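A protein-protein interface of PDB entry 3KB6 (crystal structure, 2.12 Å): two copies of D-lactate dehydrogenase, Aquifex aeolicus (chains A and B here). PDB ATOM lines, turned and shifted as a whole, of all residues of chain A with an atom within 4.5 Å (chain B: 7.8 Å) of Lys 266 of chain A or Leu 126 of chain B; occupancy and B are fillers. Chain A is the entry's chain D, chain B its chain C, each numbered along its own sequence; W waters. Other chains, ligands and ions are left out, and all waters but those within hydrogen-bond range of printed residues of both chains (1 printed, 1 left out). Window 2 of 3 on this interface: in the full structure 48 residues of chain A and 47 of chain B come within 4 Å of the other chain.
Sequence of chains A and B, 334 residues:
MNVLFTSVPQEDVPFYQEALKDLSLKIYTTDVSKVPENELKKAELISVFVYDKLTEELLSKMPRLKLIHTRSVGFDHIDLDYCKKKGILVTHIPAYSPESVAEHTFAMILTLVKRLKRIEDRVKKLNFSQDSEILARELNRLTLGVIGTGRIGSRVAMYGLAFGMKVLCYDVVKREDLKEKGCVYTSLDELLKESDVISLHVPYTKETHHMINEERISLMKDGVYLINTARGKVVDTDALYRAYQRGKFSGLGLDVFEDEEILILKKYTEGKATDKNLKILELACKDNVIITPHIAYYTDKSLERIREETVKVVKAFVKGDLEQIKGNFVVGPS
The side-chain amino group (NZ) of Lys 266 of chain A lies within hydrogen-bond range of the side-chain hydroxyl (OH) of Tyr 268 of chain A (2.6 Å). The backbone carbonyl oxygen of Lys 266 of chain A lies within hydrogen-bond range of the side-chain hydroxyl of Thr 269 of chain A, 3.0 Å away.
Hydrophobic or aromatic side chains of chain A within 4 Å of the printed part of chain B: Leu 263, Ile 264 and Leu 281. Of the 10 printed residues of chain B, 2 touch a printed residue of chain A. Hydrophobic or aromatic side chains of chain B that line the printed part of chain A: Leu 126 and Phe 128. Among the printed residues, no Asp or Glu carboxylate lies within 4 Å of a Lys or Arg side-chain nitrogen of the other chain.
Printed residues of chain B within 4 Å of Leu 263 of chain A: Phe 128 (3.6 Å). Lys 266 of chain A touches just one residue of chain B: Leu 126. Of the printed residues of chain B, Leu 281 of chain A touches Leu 126 (3.7 Å) and Phe 128 (3.8 Å). Lys 125 of chain B touches none of the printed residues of chain A. Leu 126 of chain B touches just these residues of chain A: Lys 266 and Leu 281. Of the printed residues of chain A, Phe 128 of chain B touches Leu 263, Ile 264 and Leu 281. The nearest residue of chain A that does not touch Leu 126 of chain B is Tyr 268 of chain A (4.2 Å). The nearest printed residue of chain B that does not touch Ile 264 of chain A is Ser 129 of chain B (4.05 Å).
Water W1 lies within hydrogen-bond range of O of Lys 125 of chain B (2.6 Å), O of Leu 126 of chain B (2.9 Å), NZ of Lys 266 of chain A (3.1 Å) and N of Asn 127 of chain B (3.2 Å).
The backbone carbonyl oxygen of Leu 126 of chain B lies within hydrogen-bond range of the side-chain amino group of Lys 266 of chain A, at 2.7 Å.
CB of Phe 128 of chain B touches O of Leu 263 of chain A, 3.6 Å away. Phe 128 of chain B touches Ile 264 of chain A. Leu 126 of chain B touches Leu 281 of chain A (CD1 to CD2, 3.7 Å). CD2 of Leu 281 of chain A touches CZ of Phe 128 of chain B, at 3.8 Å.
No position is printed for both chains.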
ATOM      1  N   GLU A 261     -15.475  20.025  -4.729  1.00  0.00           N
ATOM      2  CA  GLU A 261     -15.075  19.553  -3.405  1.00  0.00           C
ATOM      3  C   GLU A 261     -14.037  18.427  -3.411  1.00  0.00           C
ATOM      4  O   GLU A 261     -13.297  18.233  -2.424  1.00  0.00           O
ATOM      5  CB  GLU A 261     -16.279  19.208  -2.531  1.00  0.00           C
ATOM      6  CG  GLU A 261     -17.015  17.931  -2.838  1.00  0.00           C
ATOM      7  CD  GLU A 261     -17.778  17.964  -4.161  1.00  0.00           C
ATOM      8  OE1 GLU A 261     -17.979  19.059  -4.746  1.00  0.00           O
ATOM      9  OE2 GLU A 261     -18.172  16.866  -4.614  1.00  0.00           O
ATOM     10  N   ILE A 262     -13.956  17.729  -4.539  1.00  0.00           N
ATOM     11  CA  ILE A 262     -12.996  16.642  -4.701  1.00  0.00           C
ATOM     12  C   ILE A 262     -11.579  17.182  -4.696  1.00  0.00           C
ATOM     13  O   ILE A 262     -10.702  16.588  -4.074  1.00  0.00           O
ATOM     14  CB  ILE A 262     -13.260  15.823  -5.960  1.00  0.00           C
ATOM     15  CG1 ILE A 262     -14.584  15.029  -5.825  1.00  0.00           C
ATOM     16  CG2 ILE A 262     -12.088  14.834  -6.205  1.00  0.00           C
ATOM     17  CD1 ILE A 262     -15.147  14.507  -7.193  1.00  0.00           C
ATOM     18  N   LEU A 263     -11.383  18.313  -5.366  1.00  0.00           N
ATOM     19  CA  LEU A 263     -10.106  19.055  -5.375  1.00  0.00           C
ATOM     20  C   LEU A 263      -9.876  19.853  -4.120  1.00  0.00           C
ATOM     21  O   LEU A 263      -8.776  19.824  -3.536  1.00  0.00           O
ATOM     22  CB  LEU A 263     -10.054  20.009  -6.578  1.00  0.00           C
ATOM     23  CG  LEU A 263     -10.182  19.353  -7.922  1.00  0.00           C
ATOM     24  CD1 LEU A 263     -10.214  20.338  -9.113  1.00  0.00           C
ATOM     25  CD2 LEU A 263      -8.998  18.344  -8.076  1.00  0.00           C
ATOM     26  N   ILE A 264     -10.900  20.601  -3.694  1.00  0.00           N
ATOM     27  CA  ILE A 264     -10.747  21.470  -2.523  1.00  0.00           C
ATOM     28  C   ILE A 264     -10.450  20.690  -1.248  1.00  0.00           C
ATOM     29  O   ILE A 264      -9.658  21.127  -0.439  1.00  0.00           O
ATOM     30  CB  ILE A 264     -11.951  22.436  -2.355  1.00  0.00           C
ATOM     31  CG1 ILE A 264     -11.914  23.503  -3.445  1.00  0.00           C
ATOM     32  CG2 ILE A 264     -11.933  23.110  -0.976  1.00  0.00           C
ATOM     33  CD1 ILE A 264     -13.215  24.174  -3.650  1.00  0.00           C
ATOM     34  N   LEU A 265     -11.071  19.530  -1.079  1.00  0.00           N
ATOM     35  CA  LEU A 265     -10.847  18.695   0.112  1.00  0.00           C
ATOM     36  C   LEU A 265      -9.982  17.470  -0.190  1.00  0.00           C
ATOM     37  O   LEU A 265      -9.910  16.587   0.630  1.00  0.00           O
ATOM     38  CB  LEU A 265     -12.179  18.202   0.699  1.00  0.00           C
ATOM     39  CG  LEU A 265     -13.163  19.267   1.164  1.00  0.00           C
ATOM     40  CD1 LEU A 265     -14.405  18.607   1.732  1.00  0.00           C
ATOM     41  CD2 LEU A 265     -12.510  20.165   2.177  1.00  0.00           C
ATOM     42  N   LYS A 266      -9.343  17.417  -1.359  1.00  0.00           N
ATOM     43  CA  LYS A 266      -8.506  16.268  -1.749  1.00  0.00           C
ATOM     44  C   LYS A 266      -9.203  14.929  -1.508  1.00  0.00           C
ATOM     45  O   LYS A 266      -8.600  14.018  -0.906  1.00  0.00           O
ATOM     46  CB  LYS A 266      -7.138  16.277  -0.997  1.00  0.00           C
ATOM     47  CG  LYS A 266      -6.210  17.437  -1.393  1.00  0.00           C
ATOM     48  CD  LYS A 266      -4.733  17.055  -1.338  1.00  0.00           C
ATOM     49  CE  LYS A 266      -3.822  18.137  -1.962  1.00  0.00           C
ATOM     50  NZ  LYS A 266      -4.164  18.540  -3.373  1.00  0.00           N
ATOM     51  N   LYS A 267     -10.449  14.792  -1.965  1.00  0.00           N
ATOM     52  CA  LYS A 267     -11.180  13.528  -1.768  1.00  0.00           C
ATOM     53  C   LYS A 267     -10.633  12.399  -2.658  1.00  0.00           C
ATOM     54  O   LYS A 267     -10.950  11.226  -2.436  1.00  0.00           O
ATOM     55  CB  LYS A 267     -12.715  13.703  -1.939  1.00  0.00           C
ATOM     56  CG  LYS A 267     -13.370  14.579  -0.847  1.00  0.00           C
ATOM     57  CD  LYS A 267     -14.804  14.967  -1.179  1.00  0.00           C
ATOM     58  CE  LYS A 267     -15.790  13.835  -0.872  1.00  0.00           C
ATOM     59  NZ  LYS A 267     -17.249  14.263  -0.870  1.00  0.00           N
ATOM     60  N   TYR A 268      -9.821  12.751  -3.654  1.00  0.00           N
ATOM     61  CA  TYR A 268      -9.077  11.742  -4.423  1.00  0.00           C
ATOM     62  C   TYR A 268      -8.091  10.917  -3.579  1.00  0.00           C
ATOM     63  O   TYR A 268      -7.676   9.850  -4.003  1.00  0.00           O
ATOM     64  CB  TYR A 268      -8.399  12.346  -5.661  1.00  0.00           C
ATOM     65  CG  TYR A 268      -7.342  13.400  -5.404  1.00  0.00           C
ATOM     66  CD1 TYR A 268      -6.008  13.054  -5.197  1.00  0.00           C
ATOM     67  CD2 TYR A 268      -7.674  14.749  -5.394  1.00  0.00           C
ATOM     68  CE1 TYR A 268      -5.038  14.030  -4.971  1.00  0.00           C
ATOM     69  CE2 TYR A 268      -6.723  15.725  -5.164  1.00  0.00           C
ATOM     70  CZ  TYR A 268      -5.412  15.369  -4.940  1.00  0.00           C
ATOM     71  OH  TYR A 268      -4.479  16.365  -4.742  1.00  0.00           O
ATOM     72  N   THR A 269      -7.763  11.357  -2.369  1.00  0.00           N
ATOM     73  CA  THR A 269      -6.983  10.519  -1.479  1.00  0.00           C
ATOM     74  C   THR A 269      -7.826   9.364  -0.939  1.00  0.00           C
ATOM     75  O   THR A 269      -7.274   8.398  -0.430  1.00  0.00           O
ATOM     76  CB  THR A 269      -6.384  11.280  -0.311  1.00  0.00           C
ATOM     77  OG1 THR A 269      -7.418  11.736   0.556  1.00  0.00           O
ATOM     78  CG2 THR A 269      -5.544  12.449  -0.783  1.00  0.00           C
ATOM     79  N   LEU A 281      -9.040  21.316 -14.322  1.00  0.00           N
ATOM     80  CA  LEU A 281      -7.585  21.375 -14.227  1.00  0.00           C
ATOM     81  C   LEU A 281      -6.971  21.749 -15.547  1.00  0.00           C
ATOM     82  O   LEU A 281      -6.042  22.552 -15.573  1.00  0.00           O
ATOM     83  CB  LEU A 281      -6.991  20.068 -13.662  1.00  0.00           C
ATOM     84  CG  LEU A 281      -7.282  19.814 -12.188  1.00  0.00           C
ATOM     85  CD1 LEU A 281      -6.769  18.418 -11.784  1.00  0.00           C
ATOM     86  CD2 LEU A 281      -6.619  20.888 -11.276  1.00  0.00           C
ATOM     87  N   GLU B 120      -3.094  31.382  -7.855  1.00  0.00           N
ATOM     88  CA  GLU B 120      -2.740  30.729  -9.112  1.00  0.00           C
ATOM     89  C   GLU B 120      -1.550  29.756  -8.929  1.00  0.00           C
ATOM     90  O   GLU B 120      -1.607  28.620  -9.423  1.00  0.00           O
ATOM     91  CB  GLU B 120      -2.379  31.775 -10.159  1.00  0.00           C
ATOM     92  CG  GLU B 120      -2.035  31.182 -11.524  1.00  0.00           C
ATOM     93  CD  GLU B 120      -1.486  32.193 -12.519  1.00  0.00           C
ATOM     94  OE1 GLU B 120      -1.477  33.401 -12.222  1.00  0.00           O
ATOM     95  OE2 GLU B 120      -1.052  31.766 -13.611  1.00  0.00           O
ATOM     96  N   ASP B 121      -0.514  30.185  -8.200  1.00  0.00           N
ATOM     97  CA  ASP B 121       0.620  29.302  -7.847  1.00  0.00           C
ATOM     98  C   ASP B 121       0.124  28.017  -7.134  1.00  0.00           C
ATOM     99  O   ASP B 121       0.650  26.917  -7.369  1.00  0.00           O
ATOM    100  CB  ASP B 121       1.623  29.960  -6.892  1.00  0.00           C
ATOM    101  CG  ASP B 121       2.383  31.126  -7.486  1.00  0.00           C
ATOM    102  OD1 ASP B 121       2.371  31.327  -8.714  1.00  0.00           O
ATOM    103  OD2 ASP B 121       3.022  31.849  -6.678  1.00  0.00           O
ATOM    104  N   ARG B 122      -0.835  28.171  -6.213  1.00  0.00           N
ATOM    105  CA  ARG B 122      -1.343  27.026  -5.459  1.00  0.00           C
ATOM    106  C   ARG B 122      -2.150  26.076  -6.354  1.00  0.00           C
ATOM    107  O   ARG B 122      -1.946  24.845  -6.316  1.00  0.00           O
ATOM    108  CB  ARG B 122      -2.154  27.484  -4.251  1.00  0.00           C
ATOM    109  CG  ARG B 122      -1.304  28.220  -3.213  1.00  0.00           C
ATOM    110  CD  ARG B 122      -2.108  29.168  -2.355  1.00  0.00           C
ATOM    111  NE  ARG B 122      -3.123  28.467  -1.560  1.00  0.00           N
ATOM    112  CZ  ARG B 122      -3.049  28.224  -0.256  1.00  0.00           C
ATOM    113  NH1 ARG B 122      -2.013  28.638   0.466  1.00  0.00           N
ATOM    114  NH2 ARG B 122      -4.036  27.581   0.351  1.00  0.00           N
ATOM    115  N   VAL B 123      -3.030  26.659  -7.164  1.00  0.00           N
ATOM    116  CA  VAL B 123      -3.858  25.926  -8.109  1.00  0.00           C
ATOM    117  C   VAL B 123      -3.013  25.147  -9.124  1.00  0.00           C
ATOM    118  O   VAL B 123      -3.337  24.001  -9.459  1.00  0.00           O
ATOM    119  CB  VAL B 123      -4.867  26.865  -8.816  1.00  0.00           C
ATOM    120  CG1 VAL B 123      -5.420  26.261 -10.079  1.00  0.00           C
ATOM    121  CG2 VAL B 123      -5.967  27.254  -7.850  1.00  0.00           C
ATOM    122  N   LYS B 124      -1.952  25.768  -9.614  1.00  0.00           N
ATOM    123  CA  LYS B 124      -0.959  25.079 -10.452  1.00  0.00           C
ATOM    124  C   LYS B 124      -0.355  23.825  -9.801  1.00  0.00           C
ATOM    125  O   LYS B 124      -0.012  22.886 -10.504  1.00  0.00           O
ATOM    126  CB  LYS B 124       0.188  26.026 -10.819  1.00  0.00           C
ATOM    127  CG  LYS B 124      -0.062  26.815 -12.121  1.00  0.00           C
ATOM    128  CD  LYS B 124       0.771  28.103 -12.171  1.00  0.00           C
ATOM    129  CE  LYS B 124       2.241  27.849 -11.883  1.00  0.00           C
ATOM    130  NZ  LYS B 124       3.032  29.090 -11.989  1.00  0.00           N
ATOM    131  N   LYS B 125      -0.206  23.816  -8.480  1.00  0.00           N
ATOM    132  CA  LYS B 125       0.329  22.660  -7.750  1.00  0.00           C
ATOM    133  C   LYS B 125      -0.772  21.735  -7.184  1.00  0.00           C
ATOM    134  O   LYS B 125      -0.522  20.943  -6.280  1.00  0.00           O
ATOM    135  CB  LYS B 125       1.203  23.147  -6.590  1.00  0.00           C
ATOM    136  CG  LYS B 125       2.404  23.958  -7.041  1.00  0.00           C
ATOM    137  CD  LYS B 125       3.189  24.463  -5.844  1.00  0.00           C
ATOM    138  CE  LYS B 125       4.615  24.887  -6.236  1.00  0.00           C
ATOM    139  NZ  LYS B 125       4.631  25.803  -7.405  1.00  0.00           N
ATOM    140  N   LEU B 126      -1.989  21.876  -7.707  1.00  0.00           N
ATOM    141  CA  LEU B 126      -3.141  21.138  -7.264  1.00  0.00           C
ATOM    142  C   LEU B 126      -3.476  21.368  -5.813  1.00  0.00           C
ATOM    143  O   LEU B 126      -4.083  20.510  -5.214  1.00  0.00           O
ATOM    144  CB  LEU B 126      -2.995  19.633  -7.575  1.00  0.00           C
ATOM    145  CG  LEU B 126      -3.833  19.145  -8.760  1.00  0.00           C
ATOM    146  CD1 LEU B 126      -3.268  19.769 -10.032  1.00  0.00           C
ATOM    147  CD2 LEU B 126      -3.848  17.596  -8.905  1.00  0.00           C
ATOM    148  N   ASN B 127      -3.086  22.521  -5.251  1.00  0.00           N
ATOM    149  CA  ASN B 127      -3.403  22.893  -3.882  1.00  0.00           C
ATOM    150  C   ASN B 127      -4.620  23.834  -3.960  1.00  0.00           C
ATOM    151  O   ASN B 127      -4.474  25.051  -4.192  1.00  0.00           O
ATOM    152  CB  ASN B 127      -2.215  23.583  -3.195  1.00  0.00           C
ATOM    153  CG  ASN B 127      -2.535  24.078  -1.780  1.00  0.00           C
ATOM    154  OD1 ASN B 127      -3.634  23.865  -1.252  1.00  0.00           O
ATOM    155  ND2 ASN B 127      -1.574  24.763  -1.167  1.00  0.00           N
ATOM    156  N   PHE B 128      -5.810  23.247  -3.766  1.00  0.00           N
ATOM    157  CA  PHE B 128      -7.074  23.984  -3.812  1.00  0.00           C
ATOM    158  C   PHE B 128      -7.581  24.222  -2.374  1.00  0.00           C
ATOM    159  O   PHE B 128      -8.753  24.507  -2.166  1.00  0.00           O
ATOM    160  CB  PHE B 128      -8.117  23.175  -4.605  1.00  0.00           C
ATOM    161  CG  PHE B 128      -7.997  23.295  -6.082  1.00  0.00           C
ATOM    162  CD1 PHE B 128      -9.034  23.800  -6.828  1.00  0.00           C
ATOM    163  CD2 PHE B 128      -6.872  22.871  -6.732  1.00  0.00           C
ATOM    164  CE1 PHE B 128      -8.942  23.924  -8.185  1.00  0.00           C
ATOM    165  CE2 PHE B 128      -6.761  22.995  -8.100  1.00  0.00           C
ATOM    166  CZ  PHE B 128      -7.797  23.511  -8.832  1.00  0.00           C
ATOM    167  N   SER B 129      -6.712  24.069  -1.381  1.00  0.00           N
ATOM    168  CA  SER B 129      -7.131  24.259   0.005  1.00  0.00           C
ATOM    169  C   SER B 129      -7.231  25.738   0.327  1.00  0.00           C
ATOM    170  O   SER B 129      -6.843  26.605  -0.471  1.00  0.00           O
ATOM    171  CB  SER B 129      -6.156  23.600   0.967  1.00  0.00           C
ATOM    172  OG  SER B 129      -4.958  24.324   0.985  1.00  0.00           O
HETATM  173  O   HOH W   1      -1.503  20.053  -4.014  1.00  0.00           O
